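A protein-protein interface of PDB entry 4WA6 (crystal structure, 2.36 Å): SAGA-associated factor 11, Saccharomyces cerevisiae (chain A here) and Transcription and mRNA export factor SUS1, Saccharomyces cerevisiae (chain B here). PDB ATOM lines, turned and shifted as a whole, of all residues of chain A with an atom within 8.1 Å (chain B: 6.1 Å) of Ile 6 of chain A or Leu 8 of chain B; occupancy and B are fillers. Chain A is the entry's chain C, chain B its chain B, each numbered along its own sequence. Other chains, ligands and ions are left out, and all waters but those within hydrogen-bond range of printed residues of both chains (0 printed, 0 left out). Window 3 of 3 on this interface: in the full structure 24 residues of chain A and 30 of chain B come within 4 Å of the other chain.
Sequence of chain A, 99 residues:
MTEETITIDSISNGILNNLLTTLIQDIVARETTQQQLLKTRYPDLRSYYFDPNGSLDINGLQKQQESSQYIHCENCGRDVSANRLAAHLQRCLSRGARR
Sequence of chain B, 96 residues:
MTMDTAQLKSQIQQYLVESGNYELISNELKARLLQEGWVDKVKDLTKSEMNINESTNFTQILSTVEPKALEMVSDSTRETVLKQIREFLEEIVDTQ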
ATOM      1  N   THR A   5      -9.651 -21.366  20.117  1.00  0.00           N
ATOM      2  CA  THR A   5      -9.438 -20.833  21.503  1.00  0.00           C
ATOM      3  C   THR A   5      -8.076 -21.300  22.080  1.00  0.00           C
ATOM      4  O   THR A   5      -7.091 -21.271  21.344  1.00  0.00           O
ATOM      5  CB  THR A   5     -10.622 -21.179  22.424  1.00  0.00           C
ATOM      6  OG1 THR A   5     -10.849 -22.603  22.380  1.00  0.00           O
ATOM      7  CG2 THR A   5     -11.887 -20.357  21.993  1.00  0.00           C
ATOM      8  N   ILE A   6      -7.981 -21.694  23.357  1.00  0.00           N
ATOM      9  CA  ILE A   6      -6.652 -21.885  23.930  1.00  0.00           C
ATOM     10  C   ILE A   6      -6.381 -23.289  24.405  1.00  0.00           C
ATOM     11  O   ILE A   6      -7.255 -23.944  24.923  1.00  0.00           O
ATOM     12  CB  ILE A   6      -6.312 -20.855  25.031  1.00  0.00           C
ATOM     13  CG1 ILE A   6      -7.247 -20.953  26.240  1.00  0.00           C
ATOM     14  CG2 ILE A   6      -6.321 -19.439  24.452  1.00  0.00           C
ATOM     15  CD1 ILE A   6      -6.667 -20.269  27.473  1.00  0.00           C
ATOM     16  N   THR A   7      -5.164 -23.746  24.166  1.00  0.00           N
ATOM     17  CA  THR A   7      -4.725 -25.056  24.551  1.00  0.00           C
ATOM     18  C   THR A   7      -3.335 -24.938  25.133  1.00  0.00           C
ATOM     19  O   THR A   7      -2.718 -23.873  25.108  1.00  0.00           O
ATOM     20  CB  THR A   7      -4.613 -25.941  23.336  1.00  0.00           C
ATOM     21  OG1 THR A   7      -3.596 -25.394  22.489  1.00  0.00           O
ATOM     22  CG2 THR A   7      -5.947 -26.002  22.602  1.00  0.00           C
ATOM     23  N   ILE A   8      -2.833 -26.028  25.666  1.00  0.00           N
ATOM     24  CA  ILE A   8      -1.503 -26.020  26.251  1.00  0.00           C
ATOM     25  C   ILE A   8      -0.494 -25.674  25.165  1.00  0.00           C
ATOM     26  O   ILE A   8       0.441 -24.925  25.405  1.00  0.00           O
ATOM     27  CB  ILE A   8      -1.149 -27.378  26.890  1.00  0.00           C
ATOM     28  CG1 ILE A   8      -2.162 -27.764  27.984  1.00  0.00           C
ATOM     29  CG2 ILE A   8       0.252 -27.382  27.483  1.00  0.00           C
ATOM     30  CD1 ILE A   8      -1.927 -27.051  29.291  1.00  0.00           C
ATOM     31  N   ASP A   9      -0.701 -26.196  23.958  1.00  0.00           N
ATOM     32  CA  ASP A   9       0.251 -25.960  22.882  1.00  0.00           C
ATOM     33  C   ASP A   9       0.217 -24.548  22.427  1.00  0.00           C
ATOM     34  O   ASP A   9       1.240 -23.945  22.284  1.00  0.00           O
ATOM     35  CB  ASP A   9      -0.020 -26.839  21.703  1.00  0.00           C
ATOM     36  CG  ASP A   9       0.279 -28.253  21.995  1.00  0.00           C
ATOM     37  OD1 ASP A   9       1.126 -28.503  22.892  1.00  0.00           O
ATOM     38  OD2 ASP A   9      -0.359 -29.131  21.355  1.00  0.00           O
ATOM     39  N   SER A  10      -0.970 -24.016  22.220  1.00  0.00           N
ATOM     40  CA  SER A  10      -1.066 -22.693  21.696  1.00  0.00           C
ATOM     41  C   SER A  10      -0.473 -21.709  22.693  1.00  0.00           C
ATOM     42  O   SER A  10       0.316 -20.875  22.287  1.00  0.00           O
ATOM     43  CB  SER A  10      -2.501 -22.344  21.337  1.00  0.00           C
ATOM     44  OG  SER A  10      -3.218 -21.945  22.486  1.00  0.00           O
ATOM     45  N   ILE A  11      -0.800 -21.836  23.983  1.00  0.00           N
ATOM     46  CA  ILE A  11      -0.279 -20.932  25.023  1.00  0.00           C
ATOM     47  C   ILE A  11       1.225 -21.048  25.217  1.00  0.00           C
ATOM     48  O   ILE A  11       1.918 -20.051  25.321  1.00  0.00           O
ATOM     49  CB  ILE A  11      -0.958 -21.154  26.393  1.00  0.00           C
ATOM     50  CG1 ILE A  11      -2.430 -20.826  26.338  1.00  0.00           C
ATOM     51  CG2 ILE A  11      -0.319 -20.329  27.497  1.00  0.00           C
ATOM     52  CD1 ILE A  11      -2.738 -19.372  26.224  1.00  0.00           C
ATOM     53  N   MET B   3     -15.938 -18.041  29.245  1.00  0.00           N
ATOM     54  CA  MET B   3     -14.933 -17.168  29.843  1.00  0.00           C
ATOM     55  C   MET B   3     -14.149 -16.493  28.736  1.00  0.00           C
ATOM     56  O   MET B   3     -13.974 -17.075  27.672  1.00  0.00           O
ATOM     57  CB  MET B   3     -13.969 -17.994  30.702  1.00  0.00           C
ATOM     58  CG  MET B   3     -14.090 -17.816  32.214  1.00  0.00           C
ATOM     59  SD  MET B   3     -13.100 -16.515  33.020  1.00  0.00           S
ATOM     60  CE  MET B   3     -11.802 -16.106  31.843  1.00  0.00           C
ATOM     61  N   ASP B   4     -13.662 -15.281  28.994  1.00  0.00           N
ATOM     62  CA  ASP B   4     -12.904 -14.480  28.003  1.00  0.00           C
ATOM     63  C   ASP B   4     -11.517 -15.075  27.763  1.00  0.00           C
ATOM     64  O   ASP B   4     -10.646 -14.906  28.619  1.00  0.00           O
ATOM     65  CB  ASP B   4     -12.755 -13.023  28.538  1.00  0.00           C
ATOM     66  CG  ASP B   4     -12.129 -12.046  27.523  1.00  0.00           C
ATOM     67  OD1 ASP B   4     -11.707 -12.496  26.432  1.00  0.00           O
ATOM     68  OD2 ASP B   4     -12.059 -10.808  27.829  1.00  0.00           O
ATOM     69  N   THR B   5     -11.268 -15.731  26.619  1.00  0.00           N
ATOM     70  CA  THR B   5      -9.962 -16.419  26.448  1.00  0.00           C
ATOM     71  C   THR B   5      -8.734 -15.495  26.587  1.00  0.00           C
ATOM     72  O   THR B   5      -7.700 -15.887  27.139  1.00  0.00           O
ATOM     73  CB  THR B   5      -9.854 -17.158  25.111  1.00  0.00           C
ATOM     74  OG1 THR B   5     -10.254 -16.286  24.070  1.00  0.00           O
ATOM     75  CG2 THR B   5     -10.717 -18.418  25.085  1.00  0.00           C
ATOM     76  N   ALA B   6      -8.858 -14.270  26.099  1.00  0.00           N
ATOM     77  CA  ALA B   6      -7.752 -13.296  26.133  1.00  0.00           C
ATOM     78  C   ALA B   6      -7.275 -13.007  27.551  1.00  0.00           C
ATOM     79  O   ALA B   6      -6.079 -13.029  27.836  1.00  0.00           O
ATOM     80  CB  ALA B   6      -8.201 -11.995  25.488  1.00  0.00           C
ATOM     81  N   GLN B   7      -8.237 -12.696  28.414  1.00  0.00           N
ATOM     82  CA  GLN B   7      -8.016 -12.503  29.837  1.00  0.00           C
ATOM     83  C   GLN B   7      -7.440 -13.749  30.537  1.00  0.00           C
ATOM     84  O   GLN B   7      -6.530 -13.666  31.363  1.00  0.00           O
ATOM     85  CB  GLN B   7      -9.355 -12.131  30.480  1.00  0.00           C
ATOM     86  CG  GLN B   7      -9.382 -12.193  32.001  1.00  0.00           C
ATOM     87  CD  GLN B   7     -10.601 -11.493  32.583  1.00  0.00           C
ATOM     88  OE1 GLN B   7     -11.729 -11.774  32.175  1.00  0.00           O
ATOM     89  NE2 GLN B   7     -10.385 -10.601  33.558  1.00  0.00           N
ATOM     90  N   LEU B   8      -8.003 -14.903  30.215  1.00  0.00           N
ATOM     91  CA  LEU B   8      -7.445 -16.118  30.686  1.00  0.00           C
ATOM     92  C   LEU B   8      -5.972 -16.243  30.283  1.00  0.00           C
ATOM     93  O   LEU B   8      -5.149 -16.656  31.079  1.00  0.00           O
ATOM     94  CB  LEU B   8      -8.259 -17.319  30.185  1.00  0.00           C
ATOM     95  CG  LEU B   8      -7.985 -18.674  30.831  1.00  0.00           C
ATOM     96  CD1 LEU B   8      -7.682 -18.496  32.312  1.00  0.00           C
ATOM     97  CD2 LEU B   8      -9.165 -19.632  30.637  1.00  0.00           C
ATOM     98  N   LYS B   9      -5.619 -15.892  29.056  1.00  0.00           N
ATOM     99  CA  LYS B   9      -4.208 -16.023  28.648  1.00  0.00           C
ATOM    100  C   LYS B   9      -3.322 -15.102  29.519  1.00  0.00           C
ATOM    101  O   LYS B   9      -2.246 -15.456  29.968  1.00  0.00           O
ATOM    102  CB  LYS B   9      -4.079 -15.707  27.190  1.00  0.00           C
ATOM    103  CG  LYS B   9      -2.666 -15.813  26.666  1.00  0.00           C
ATOM    104  CD  LYS B   9      -2.639 -15.204  25.274  1.00  0.00           C
ATOM    105  CE  LYS B   9      -3.330 -16.132  24.281  1.00  0.00           C
ATOM    106  NZ  LYS B   9      -3.955 -15.342  23.199  1.00  0.00           N
ATOM    107  N   SER B  10      -3.860 -13.949  29.833  1.00  0.00           N
ATOM    108  CA  SER B  10      -3.236 -13.032  30.757  1.00  0.00           C
ATOM    109  C   SER B  10      -3.081 -13.526  32.193  1.00  0.00           C
ATOM    110  O   SER B  10      -2.060 -13.271  32.811  1.00  0.00           O
ATOM    111  CB  SER B  10      -4.069 -11.759  30.784  1.00  0.00           C
ATOM    112  OG  SER B  10      -3.203 -10.696  31.051  1.00  0.00           O
ATOM    113  N   GLN B  11      -4.076 -14.229  32.745  1.00  0.00           N
ATOM    114  CA  GLN B  11      -3.913 -14.798  34.085  1.00  0.00           C
ATOM    115  C   GLN B  11      -2.818 -15.848  34.064  1.00  0.00           C
ATOM    116  O   GLN B  11      -1.975 -15.895  34.981  1.00  0.00           O
ATOM    117  CB  GLN B  11      -5.210 -15.440  34.620  1.00  0.00           C
ATOM    118  CG  GLN B  11      -6.265 -14.446  35.098  1.00  0.00           C
ATOM    119  CD  GLN B  11      -7.700 -14.895  34.849  1.00  0.00           C
ATOM    120  OE1 GLN B  11      -7.986 -16.087  34.696  1.00  0.00           O
ATOM    121  NE2 GLN B  11      -8.620 -13.921  34.811  1.00  0.00           N
ATOM    122  N   ILE B  12      -2.803 -16.673  33.021  1.00  0.00           N
ATOM    123  CA  ILE B  12      -1.846 -17.751  32.993  1.00  0.00           C
ATOM    124  C   ILE B  12      -0.407 -17.185  33.069  1.00  0.00           C
ATOM    125  O   ILE B  12       0.408 -17.568  33.935  1.00  0.00           O
ATOM    126  CB  ILE B  12      -2.092 -18.655  31.778  1.00  0.00           C
ATOM    127  CG1 ILE B  12      -3.413 -19.411  31.925  1.00  0.00           C
ATOM    128  CG2 ILE B  12      -1.000 -19.682  31.637  1.00  0.00           C
ATOM    129  CD1 ILE B  12      -3.762 -20.273  30.723  1.00  0.00           C
ATOM    130  N   GLN B  13      -0.133 -16.205  32.208  1.00  0.00           N
ATOM    131  CA  GLN B  13       1.182 -15.557  32.164  1.00  0.00           C
ATOM    132  C   GLN B  13       1.499 -14.965  33.536  1.00  0.00           C
ATOM    133  O   GLN B  13       2.585 -15.124  34.098  1.00  0.00           O
ATOM    134  CB  GLN B  13       1.194 -14.487  31.073  1.00  0.00           C
ATOM    135  CG  GLN B  13       1.227 -15.082  29.676  1.00  0.00           C
ATOM    136  CD  GLN B  13       1.142 -14.047  28.558  1.00  0.00           C
ATOM    137  OE1 GLN B  13       1.189 -12.872  28.809  1.00  0.00           O
ATOM    138  NE2 GLN B  13       0.956 -14.504  27.322  1.00  0.00           N
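Among the printed residues, merely in contact across the chains: Ile 11 of chain A with Lys 9 of chain B (3.6 Å), Thr 5 of chain A with Thr 5 of chain B (3.8 Å) and Ile 6 of chain A with Leu 8 of chain B (3.9 Å).
Ile 6 of chain A touches one residue of chain B.
Ser 10 of chain A touches none of the printed residues of chain B.
Printed residues of chain B within 4 Å of Ile 11 of chain A: Lys 9.
Printed residues of chain A within 4 Å of Thr 5 of chain B: Thr 5 (3.8 Å).
Printed residues of chain A within 4 Å of Lys 9 of chain B: Ile 11 (3.6 Å).
The nearest residue of chain B that does not touch Ile 6 of chain A is Thr 5 of chain B (4.3 Å).
The nearest residue of chain A that does not touch Leu 8 of chain B is Ile 11 of chain A (6.1 Å).
Of the 11 printed residues of chain B, 3 touch a printed residue of chain A.
Hydrophobic or aromatic side chains of chain A that line the printed part of chain B: Ile 6 and Ile 11.
Among the printed residues, no Asp or Glu carboxylate lies within 4 Å of a Lys or Arg side-chain nitrogen of the other chain.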
